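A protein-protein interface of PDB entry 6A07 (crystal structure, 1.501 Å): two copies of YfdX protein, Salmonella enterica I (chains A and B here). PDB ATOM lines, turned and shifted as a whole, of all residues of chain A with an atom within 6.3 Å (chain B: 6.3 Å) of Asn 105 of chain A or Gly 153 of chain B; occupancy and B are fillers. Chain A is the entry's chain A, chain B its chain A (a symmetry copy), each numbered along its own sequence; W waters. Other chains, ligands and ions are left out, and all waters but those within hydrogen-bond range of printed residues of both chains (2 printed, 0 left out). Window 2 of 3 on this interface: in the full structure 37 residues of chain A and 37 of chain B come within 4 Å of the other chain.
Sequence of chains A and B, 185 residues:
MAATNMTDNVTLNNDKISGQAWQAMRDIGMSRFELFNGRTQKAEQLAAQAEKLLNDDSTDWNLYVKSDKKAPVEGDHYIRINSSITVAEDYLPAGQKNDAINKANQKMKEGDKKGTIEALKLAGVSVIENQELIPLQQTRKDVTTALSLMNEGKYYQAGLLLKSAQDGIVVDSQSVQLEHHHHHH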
ATOM      1  N   ALA A 100       3.071  -7.410  16.310  1.00  0.00           N
ATOM      2  CA  ALA A 100       4.101  -8.221  15.667  1.00  0.00           C
ATOM      3  C   ALA A 100       3.583  -9.609  15.306  1.00  0.00           C
ATOM      4  O   ALA A 100       4.016 -10.192  14.305  1.00  0.00           O
ATOM      5  CB  ALA A 100       5.323  -8.319  16.578  1.00  0.00           C
ATOM      6  N   ILE A 101       2.670 -10.154  16.113  1.00  0.00           N
ATOM      7  CA  ILE A 101       2.070 -11.441  15.783  1.00  0.00           C
ATOM      8  C   ILE A 101       1.199 -11.316  14.539  1.00  0.00           C
ATOM      9  O   ILE A 101       1.135 -12.243  13.721  1.00  0.00           O
ATOM     10  CB  ILE A 101       1.290 -11.983  16.997  1.00  0.00           C
ATOM     11  CG1 ILE A 101       2.258 -12.436  18.100  1.00  0.00           C
ATOM     12  CG2 ILE A 101       0.395 -13.141  16.604  1.00  0.00           C
ATOM     13  CD1 ILE A 101       3.239 -13.521  17.660  1.00  0.00           C
ATOM     14  N   ASN A 102       0.541 -10.168  14.349  1.00  0.00           N
ATOM     15  CA  ASN A 102      -0.240  -9.976  13.131  1.00  0.00           C
ATOM     16  C   ASN A 102       0.642 -10.047  11.888  1.00  0.00           C
ATOM     17  O   ASN A 102       0.244 -10.614  10.866  1.00  0.00           O
ATOM     18  CB  ASN A 102      -0.986  -8.648  13.185  1.00  0.00           C
ATOM     19  CG  ASN A 102      -1.788  -8.388  11.928  1.00  0.00           C
ATOM     20  OD1 ASN A 102      -2.905  -8.883  11.778  1.00  0.00           O
ATOM     21  ND2 ASN A 102      -1.217  -7.618  11.008  1.00  0.00           N
ATOM     22  N   LYS A 103       1.845  -9.471  11.952  1.00  0.00           N
ATOM     23  CA  LYS A 103       2.755  -9.573  10.816  1.00  0.00           C
ATOM     24  C   LYS A 103       3.268 -10.998  10.646  1.00  0.00           C
ATOM     25  O   LYS A 103       3.438 -11.471   9.516  1.00  0.00           O
ATOM     26  CB  LYS A 103       3.916  -8.589  10.983  1.00  0.00           C
ATOM     27  CG  LYS A 103       5.019  -8.762   9.948  1.00  0.00           C
ATOM     28  CD  LYS A 103       6.194  -7.828  10.199  1.00  0.00           C
ATOM     29  CE  LYS A 103       7.230  -7.969   9.101  1.00  0.00           C
ATOM     30  NZ  LYS A 103       8.233  -9.016   9.435  1.00  0.00           N
ATOM     31  N   ALA A 104       3.533 -11.695  11.753  1.00  0.00           N
ATOM     32  CA  ALA A 104       3.922 -13.096  11.642  1.00  0.00           C
ATOM     33  C   ALA A 104       2.839 -13.909  10.944  1.00  0.00           C
ATOM     34  O   ALA A 104       3.139 -14.769  10.105  1.00  0.00           O
ATOM     35  CB  ALA A 104       4.223 -13.666  13.029  1.00  0.00           C
ATOM     36  N   ASN A 105       1.577 -13.635  11.261  1.00  0.00           N
ATOM     37  CA  ASN A 105       0.483 -14.373  10.640  1.00  0.00           C
ATOM     38  C   ASN A 105       0.444 -14.147   9.133  1.00  0.00           C
ATOM     39  O   ASN A 105       0.156 -15.074   8.367  1.00  0.00           O
ATOM     40  CB  ASN A 105      -0.832 -13.982  11.299  1.00  0.00           C
ATOM     41  CG  ASN A 105      -1.022 -14.677  12.636  1.00  0.00           C
ATOM     42  OD1 ASN A 105      -0.431 -15.728  12.864  1.00  0.00           O
ATOM     43  ND2 ASN A 105      -1.844 -14.108  13.506  1.00  0.00           N
ATOM     44  N   GLN A 106       0.771 -12.935   8.685  1.00  0.00           N
ATOM     45  CA  GLN A 106       0.817 -12.672   7.250  1.00  0.00           C
ATOM     46  C   GLN A 106       1.898 -13.496   6.561  1.00  0.00           C
ATOM     47  O   GLN A 106       1.675 -14.042   5.476  1.00  0.00           O
ATOM     48  CB  GLN A 106       1.043 -11.180   7.004  1.00  0.00           C
ATOM     49  CG  GLN A 106       1.222 -10.821   5.543  1.00  0.00           C
ATOM     50  CD  GLN A 106      -0.062 -10.960   4.751  1.00  0.00           C
ATOM     51  OE1 GLN A 106      -1.155 -10.729   5.276  1.00  0.00           O
ATOM     52  NE2 GLN A 106       0.062 -11.337   3.479  1.00  0.00           N
ATOM     53  N   LYS A 107       3.076 -13.612   7.183  1.00  0.00           N
ATOM     54  CA  LYS A 107       4.164 -14.368   6.574  1.00  0.00           C
ATOM     55  C   LYS A 107       3.835 -15.854   6.495  1.00  0.00           C
ATOM     56  O   LYS A 107       4.210 -16.526   5.526  1.00  0.00           O
ATOM     57  CB  LYS A 107       5.457 -14.142   7.357  1.00  0.00           C
ATOM     58  CG  LYS A 107       5.860 -12.685   7.434  1.00  0.00           C
ATOM     59  CD  LYS A 107       6.056 -12.100   6.038  1.00  0.00           C
ATOM     60  CE  LYS A 107       6.335 -10.606   6.105  1.00  0.00           C
ATOM     61  NZ  LYS A 107       6.769 -10.069   4.784  1.00  0.00           N
ATOM     62  N   MET A 108       3.147 -16.393   7.506  1.00  0.00           N
ATOM     63  CA  MET A 108       2.732 -17.791   7.430  1.00  0.00           C
ATOM     64  C   MET A 108       1.714 -18.000   6.315  1.00  0.00           C
ATOM     65  O   MET A 108       1.798 -18.981   5.569  1.00  0.00           O
ATOM     66  CB  MET A 108       2.168 -18.248   8.773  1.00  0.00           C
ATOM     67  CG  MET A 108       3.253 -18.611   9.761  1.00  0.00           C
ATOM     68  SD  MET A 108       2.611 -19.211  11.336  1.00  0.00           S
ATOM     69  CE  MET A 108       2.269 -17.650  12.143  1.00  0.00           C
ATOM     70  N   LYS A 109       0.757 -17.079   6.187  1.00  0.00           N
ATOM     71  CA  LYS A 109      -0.178 -17.112   5.066  1.00  0.00           C
ATOM     72  C   LYS A 109       0.550 -17.187   3.726  1.00  0.00           C
ATOM     73  O   LYS A 109       0.128 -17.917   2.824  1.00  0.00           O
ATOM     74  CB  LYS A 109      -1.082 -15.880   5.107  1.00  0.00           C
ATOM     75  CG  LYS A 109      -2.069 -15.806   3.937  1.00  0.00           C
ATOM     76  CD  LYS A 109      -2.603 -14.395   3.723  1.00  0.00           C
ATOM     77  CE  LYS A 109      -3.476 -13.934   4.874  1.00  0.00           C
ATOM     78  NZ  LYS A 109      -4.482 -12.939   4.397  1.00  0.00           N
ATOM     79  N   GLU A 110       1.647 -16.443   3.582  1.00  0.00           N
ATOM     80  CA  GLU A 110       2.372 -16.375   2.318  1.00  0.00           C
ATOM     81  C   GLU A 110       3.306 -17.556   2.085  1.00  0.00           C
ATOM     82  O   GLU A 110       3.889 -17.653   0.998  1.00  0.00           O
ATOM     83  CB  GLU A 110       3.164 -15.063   2.246  1.00  0.00           C
ATOM     84  CG  GLU A 110       2.270 -13.831   2.277  1.00  0.00           C
ATOM     85  CD  GLU A 110       3.035 -12.530   2.427  1.00  0.00           C
ATOM     86  OE1 GLU A 110       4.273 -12.566   2.595  1.00  0.00           O
ATOM     87  OE2 GLU A 110       2.385 -11.464   2.385  1.00  0.00           O
ATOM     88  N   ALA A 119       9.607 -12.262  11.602  1.00  0.00           N
ATOM     89  CA  ALA A 119       8.503 -11.554  12.237  1.00  0.00           C
ATOM     90  C   ALA A 119       8.286 -12.041  13.661  1.00  0.00           C
ATOM     91  O   ALA A 119       7.986 -11.246  14.562  1.00  0.00           O
ATOM     92  CB  ALA A 119       7.226 -11.723  11.412  1.00  0.00           C
ATOM     93  N   THR B  40      -0.037 -23.351   5.691  1.00  0.00           N
ATOM     94  CA  THR B  40      -1.242 -23.178   6.503  1.00  0.00           C
ATOM     95  C   THR B  40      -2.426 -23.952   5.940  1.00  0.00           C
ATOM     96  O   THR B  40      -3.290 -24.391   6.704  1.00  0.00           O
ATOM     97  CB  THR B  40      -1.617 -21.698   6.651  1.00  0.00           C
ATOM     98  OG1 THR B  40      -1.855 -21.123   5.357  1.00  0.00           O
ATOM     99  CG2 THR B  40      -0.529 -20.936   7.380  1.00  0.00           C
ATOM    100  N   SER B 148     -11.252 -22.307  13.405  1.00  0.00           N
ATOM    101  CA  SER B 148     -11.878 -20.997  13.249  1.00  0.00           C
ATOM    102  C   SER B 148     -10.831 -19.894  13.206  1.00  0.00           C
ATOM    103  O   SER B 148     -10.912 -18.979  12.378  1.00  0.00           O
ATOM    104  CB  SER B 148     -12.871 -20.752  14.382  1.00  0.00           C
ATOM    105  OG  SER B 148     -14.007 -21.590  14.257  1.00  0.00           O
ATOM    106  N   LEU B 149      -9.823 -19.972  14.077  1.00  0.00           N
ATOM    107  CA  LEU B 149      -8.743 -18.992  14.041  1.00  0.00           C
ATOM    108  C   LEU B 149      -7.976 -19.072  12.729  1.00  0.00           C
ATOM    109  O   LEU B 149      -7.575 -18.043  12.169  1.00  0.00           O
ATOM    110  CB  LEU B 149      -7.797 -19.209  15.227  1.00  0.00           C
ATOM    111  CG  LEU B 149      -8.403 -18.855  16.589  1.00  0.00           C
ATOM    112  CD1 LEU B 149      -7.584 -19.455  17.728  1.00  0.00           C
ATOM    113  CD2 LEU B 149      -8.503 -17.333  16.763  1.00  0.00           C
ATOM    114  N   MET B 150      -7.740 -20.291  12.230  1.00  0.00           N
ATOM    115  CA  MET B 150      -7.085 -20.431  10.934  1.00  0.00           C
ATOM    116  C   MET B 150      -7.928 -19.794   9.831  1.00  0.00           C
ATOM    117  O   MET B 150      -7.386 -19.101   8.960  1.00  0.00           O
ATOM    118  CB  MET B 150      -6.804 -21.903  10.635  1.00  0.00           C
ATOM    119  CG  MET B 150      -5.736 -22.520  11.543  1.00  0.00           C
ATOM    120  SD  MET B 150      -5.465 -24.233  11.063  1.00  0.00           S
ATOM    121  CE  MET B 150      -4.829 -24.888  12.611  1.00  0.00           C
ATOM    122  N   ASN B 151      -9.252 -19.979   9.879  1.00  0.00           N
ATOM    123  CA  ASN B 151     -10.124 -19.331   8.895  1.00  0.00           C
ATOM    124  C   ASN B 151      -9.964 -17.819   8.929  1.00  0.00           C
ATOM    125  O   ASN B 151     -10.007 -17.155   7.886  1.00  0.00           O
ATOM    126  CB  ASN B 151     -11.589 -19.694   9.148  1.00  0.00           C
ATOM    127  CG  ASN B 151     -11.894 -21.148   8.879  1.00  0.00           C
ATOM    128  OD1 ASN B 151     -11.181 -21.819   8.146  1.00  0.00           O
ATOM    129  ND2 ASN B 151     -12.969 -21.637   9.476  1.00  0.00           N
ATOM    130  N   GLU B 152      -9.813 -17.253  10.122  1.00  0.00           N
ATOM    131  CA  GLU B 152      -9.643 -15.815  10.289  1.00  0.00           C
ATOM    132  C   GLU B 152      -8.232 -15.337   9.975  1.00  0.00           C
ATOM    133  O   GLU B 152      -7.988 -14.124  10.005  1.00  0.00           O
ATOM    134  CB  GLU B 152     -10.010 -15.415  11.717  1.00  0.00           C
ATOM    135  CG  GLU B 152     -11.414 -15.774  12.136  1.00  0.00           C
ATOM    136  CD  GLU B 152     -11.651 -15.525  13.616  1.00  0.00           C
ATOM    137  OE1 GLU B 152     -10.702 -15.097  14.302  1.00  0.00           O
ATOM    138  OE2 GLU B 152     -12.778 -15.757  14.091  1.00  0.00           O
ATOM    139  N   GLY B 153      -7.295 -16.242   9.702  1.00  0.00           N
ATOM    140  CA  GLY B 153      -5.926 -15.846   9.472  1.00  0.00           C
ATOM    141  C   GLY B 153      -5.083 -15.694  10.719  1.00  0.00           C
ATOM    142  O   GLY B 153      -3.952 -15.207  10.622  1.00  0.00           O
ATOM    143  N   LYS B 154      -5.602 -16.080  11.886  1.00  0.00           N
ATOM    144  CA  LYS B 154      -4.860 -15.941  13.147  1.00  0.00           C
ATOM    145  C   LYS B 154      -4.091 -17.238  13.428  1.00  0.00           C
ATOM    146  O   LYS B 154      -4.417 -18.020  14.322  1.00  0.00           O
ATOM    147  CB  LYS B 154      -5.813 -15.586  14.282  1.00  0.00           C
ATOM    148  CG  LYS B 154      -6.492 -14.214  14.136  1.00  0.00           C
ATOM    149  CD  LYS B 154      -7.317 -13.859  15.369  1.00  0.00           C
ATOM    150  CE  LYS B 154      -7.762 -12.405  15.337  1.00  0.00           C
ATOM    151  NZ  LYS B 154      -9.068 -12.299  14.647  1.00  0.00           N
ATOM    152  N   TYR B 155      -3.042 -17.452  12.630  1.00  0.00           N
ATOM    153  CA  TYR B 155      -2.374 -18.754  12.620  1.00  0.00           C
ATOM    154  C   TYR B 155      -1.574 -18.992  13.897  1.00  0.00           C
ATOM    155  O   TYR B 155      -1.600 -20.106  14.444  1.00  0.00           O
ATOM    156  CB  TYR B 155      -1.483 -18.869  11.390  1.00  0.00           C
ATOM    157  CG  TYR B 155      -2.266 -18.757  10.100  1.00  0.00           C
ATOM    158  CD1 TYR B 155      -3.171 -19.739   9.737  1.00  0.00           C
ATOM    159  CD2 TYR B 155      -2.098 -17.669   9.253  1.00  0.00           C
ATOM    160  CE1 TYR B 155      -3.895 -19.646   8.559  1.00  0.00           C
ATOM    161  CE2 TYR B 155      -2.819 -17.569   8.077  1.00  0.00           C
ATOM    162  CZ  TYR B 155      -3.715 -18.561   7.744  1.00  0.00           C
ATOM    163  OH  TYR B 155      -4.447 -18.485   6.571  1.00  0.00           O
ATOM    164  N   TYR B 156      -0.860 -17.976  14.388  1.00  0.00           N
ATOM    165  CA  TYR B 156      -0.095 -18.173  15.620  1.00  0.00           C
ATOM    166  C   TYR B 156      -1.022 -18.521  16.779  1.00  0.00           C
ATOM    167  O   TYR B 156      -0.731 -19.423  17.581  1.00  0.00           O
ATOM    168  CB  TYR B 156       0.722 -16.919  15.947  1.00  0.00           C
ATOM    169  CG  TYR B 156       1.717 -17.165  17.049  1.00  0.00           C
ATOM    170  CD1 TYR B 156       2.931 -17.783  16.779  1.00  0.00           C
ATOM    171  CD2 TYR B 156       1.438 -16.793  18.358  1.00  0.00           C
ATOM    172  CE1 TYR B 156       3.853 -18.025  17.795  1.00  0.00           C
ATOM    173  CE2 TYR B 156       2.346 -17.031  19.376  1.00  0.00           C
ATOM    174  CZ  TYR B 156       3.547 -17.648  19.082  1.00  0.00           C
ATOM    175  OH  TYR B 156       4.463 -17.888  20.093  1.00  0.00           O
ATOM    176  N   GLN B 157      -2.158 -17.824  16.876  1.00  0.00           N
ATOM    177  CA  GLN B 157      -3.120 -18.115  17.928  1.00  0.00           C
ATOM    178  C   GLN B 157      -3.683 -19.530  17.788  1.00  0.00           C
ATOM    179  O   GLN B 157      -3.883 -20.226  18.790  1.00  0.00           O
ATOM    180  CB  GLN B 157      -4.241 -17.075  17.902  1.00  0.00           C
ATOM    181  CG  GLN B 157      -3.763 -15.629  18.167  1.00  0.00           C
ATOM    182  CD  GLN B 157      -3.453 -14.849  16.894  1.00  0.00           C
ATOM    183  OE1 GLN B 157      -2.861 -15.364  15.952  1.00  0.00           O
ATOM    184  NE2 GLN B 157      -3.857 -13.578  16.876  1.00  0.00           N
HETATM  185  O   HOH W   1       0.799 -21.009   4.005  1.00  0.00           O
HETATM  186  O   HOH W   2      -2.981 -13.607   8.301  1.00  0.00           O
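Printed residues of chain B within 4 Å of Ile 101 of chain A: Tyr 156 and Gln 157. Lys 103 of chain A touches none of the printed residues of chain B. Of the printed residues of chain B, Asn 105 of chain A touches Gly 153, Lys 154, Tyr 155, Tyr 156 and Gln 157. Printed residues of chain B within 4 Å of Met 108 of chain A: Thr 40 and Tyr 156. Of the printed residues of chain A, Gly 153 of chain B touches Asn 105 (3.4 Å). Of the printed residues of chain A, Gln 157 of chain B touches Ile 101 (3.996 Å) and Asn 105 (2.9 Å). The nearest residue of chain B that does not touch Asn 105 of chain A is Thr 40 of chain B (6.0 Å). The nearest printed residue of chain A that does not touch Gln 157 of chain B is Asn 102 of chain A (6.1 Å).
No position is printed for both chains.
Among the printed residues, merely in contact across the chains: Asn 105 of chain A with Gly 153 of chain B (3.4 Å), Met 108 of chain A with Thr 40 of chain B (3.5 Å), Asn 105 of chain A with Lys 154 of chain B (3.5 Å), Ile 101 of chain A with Tyr 156 of chain B (3.8 Å), Lys 109 of chain A with Tyr 155 of chain B (3.8 Å), Met 108 of chain A with Tyr 156 of chain B (3.9 Å) and Ile 101 of chain A with Gln 157 of chain B (3.996 Å).
The backbone carbonyl oxygen (O) of Leu 149 of chain B sits at hydrogen-bond distance from the backbone NH (N) of Lys 154 of chain B. The side-chain carboxylate (OE1) of Glu 152 of chain B lies within salt-bridge range of the side-chain amino group (NZ) of Lys 154 of chain B, at 3.3 Å. The side-chain amide oxygen of Gln 157 of chain B sits close to the backbone carbonyl oxygen of Lys 154 of chain B (3.5 Å).
Water W1 lies within hydrogen-bond range of the backbone carbonyl oxygen of Met 108 of chain A, the side-chain hydroxyl of Thr 40 of chain B and the backbone carbonyl oxygen of Lys 109 of chain A. Water W2 bridges O of Gly 153 of chain B (3.0 Å) and O of Asn 105 of chain A (3.5 Å).
N of Tyr 155 of chain B lies within hydrogen-bond range of OD1 of Asn 105 of chain A (3.1 Å). OD1 of Asn 105 of chain A is in hydrogen-bond range of N of Tyr 156 of chain B, at 2.7 Å. The side-chain amide nitrogen (ND2) of Asn 105 of chain A sits at hydrogen-bond distance from the side-chain amide oxygen (OE1) of Gln 157 of chain B (2.9 Å).
Of the 12 printed residues of chain A, 4 touch a printed residue of chain B. Among the printed residues, 10 pairs touch across the chains.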
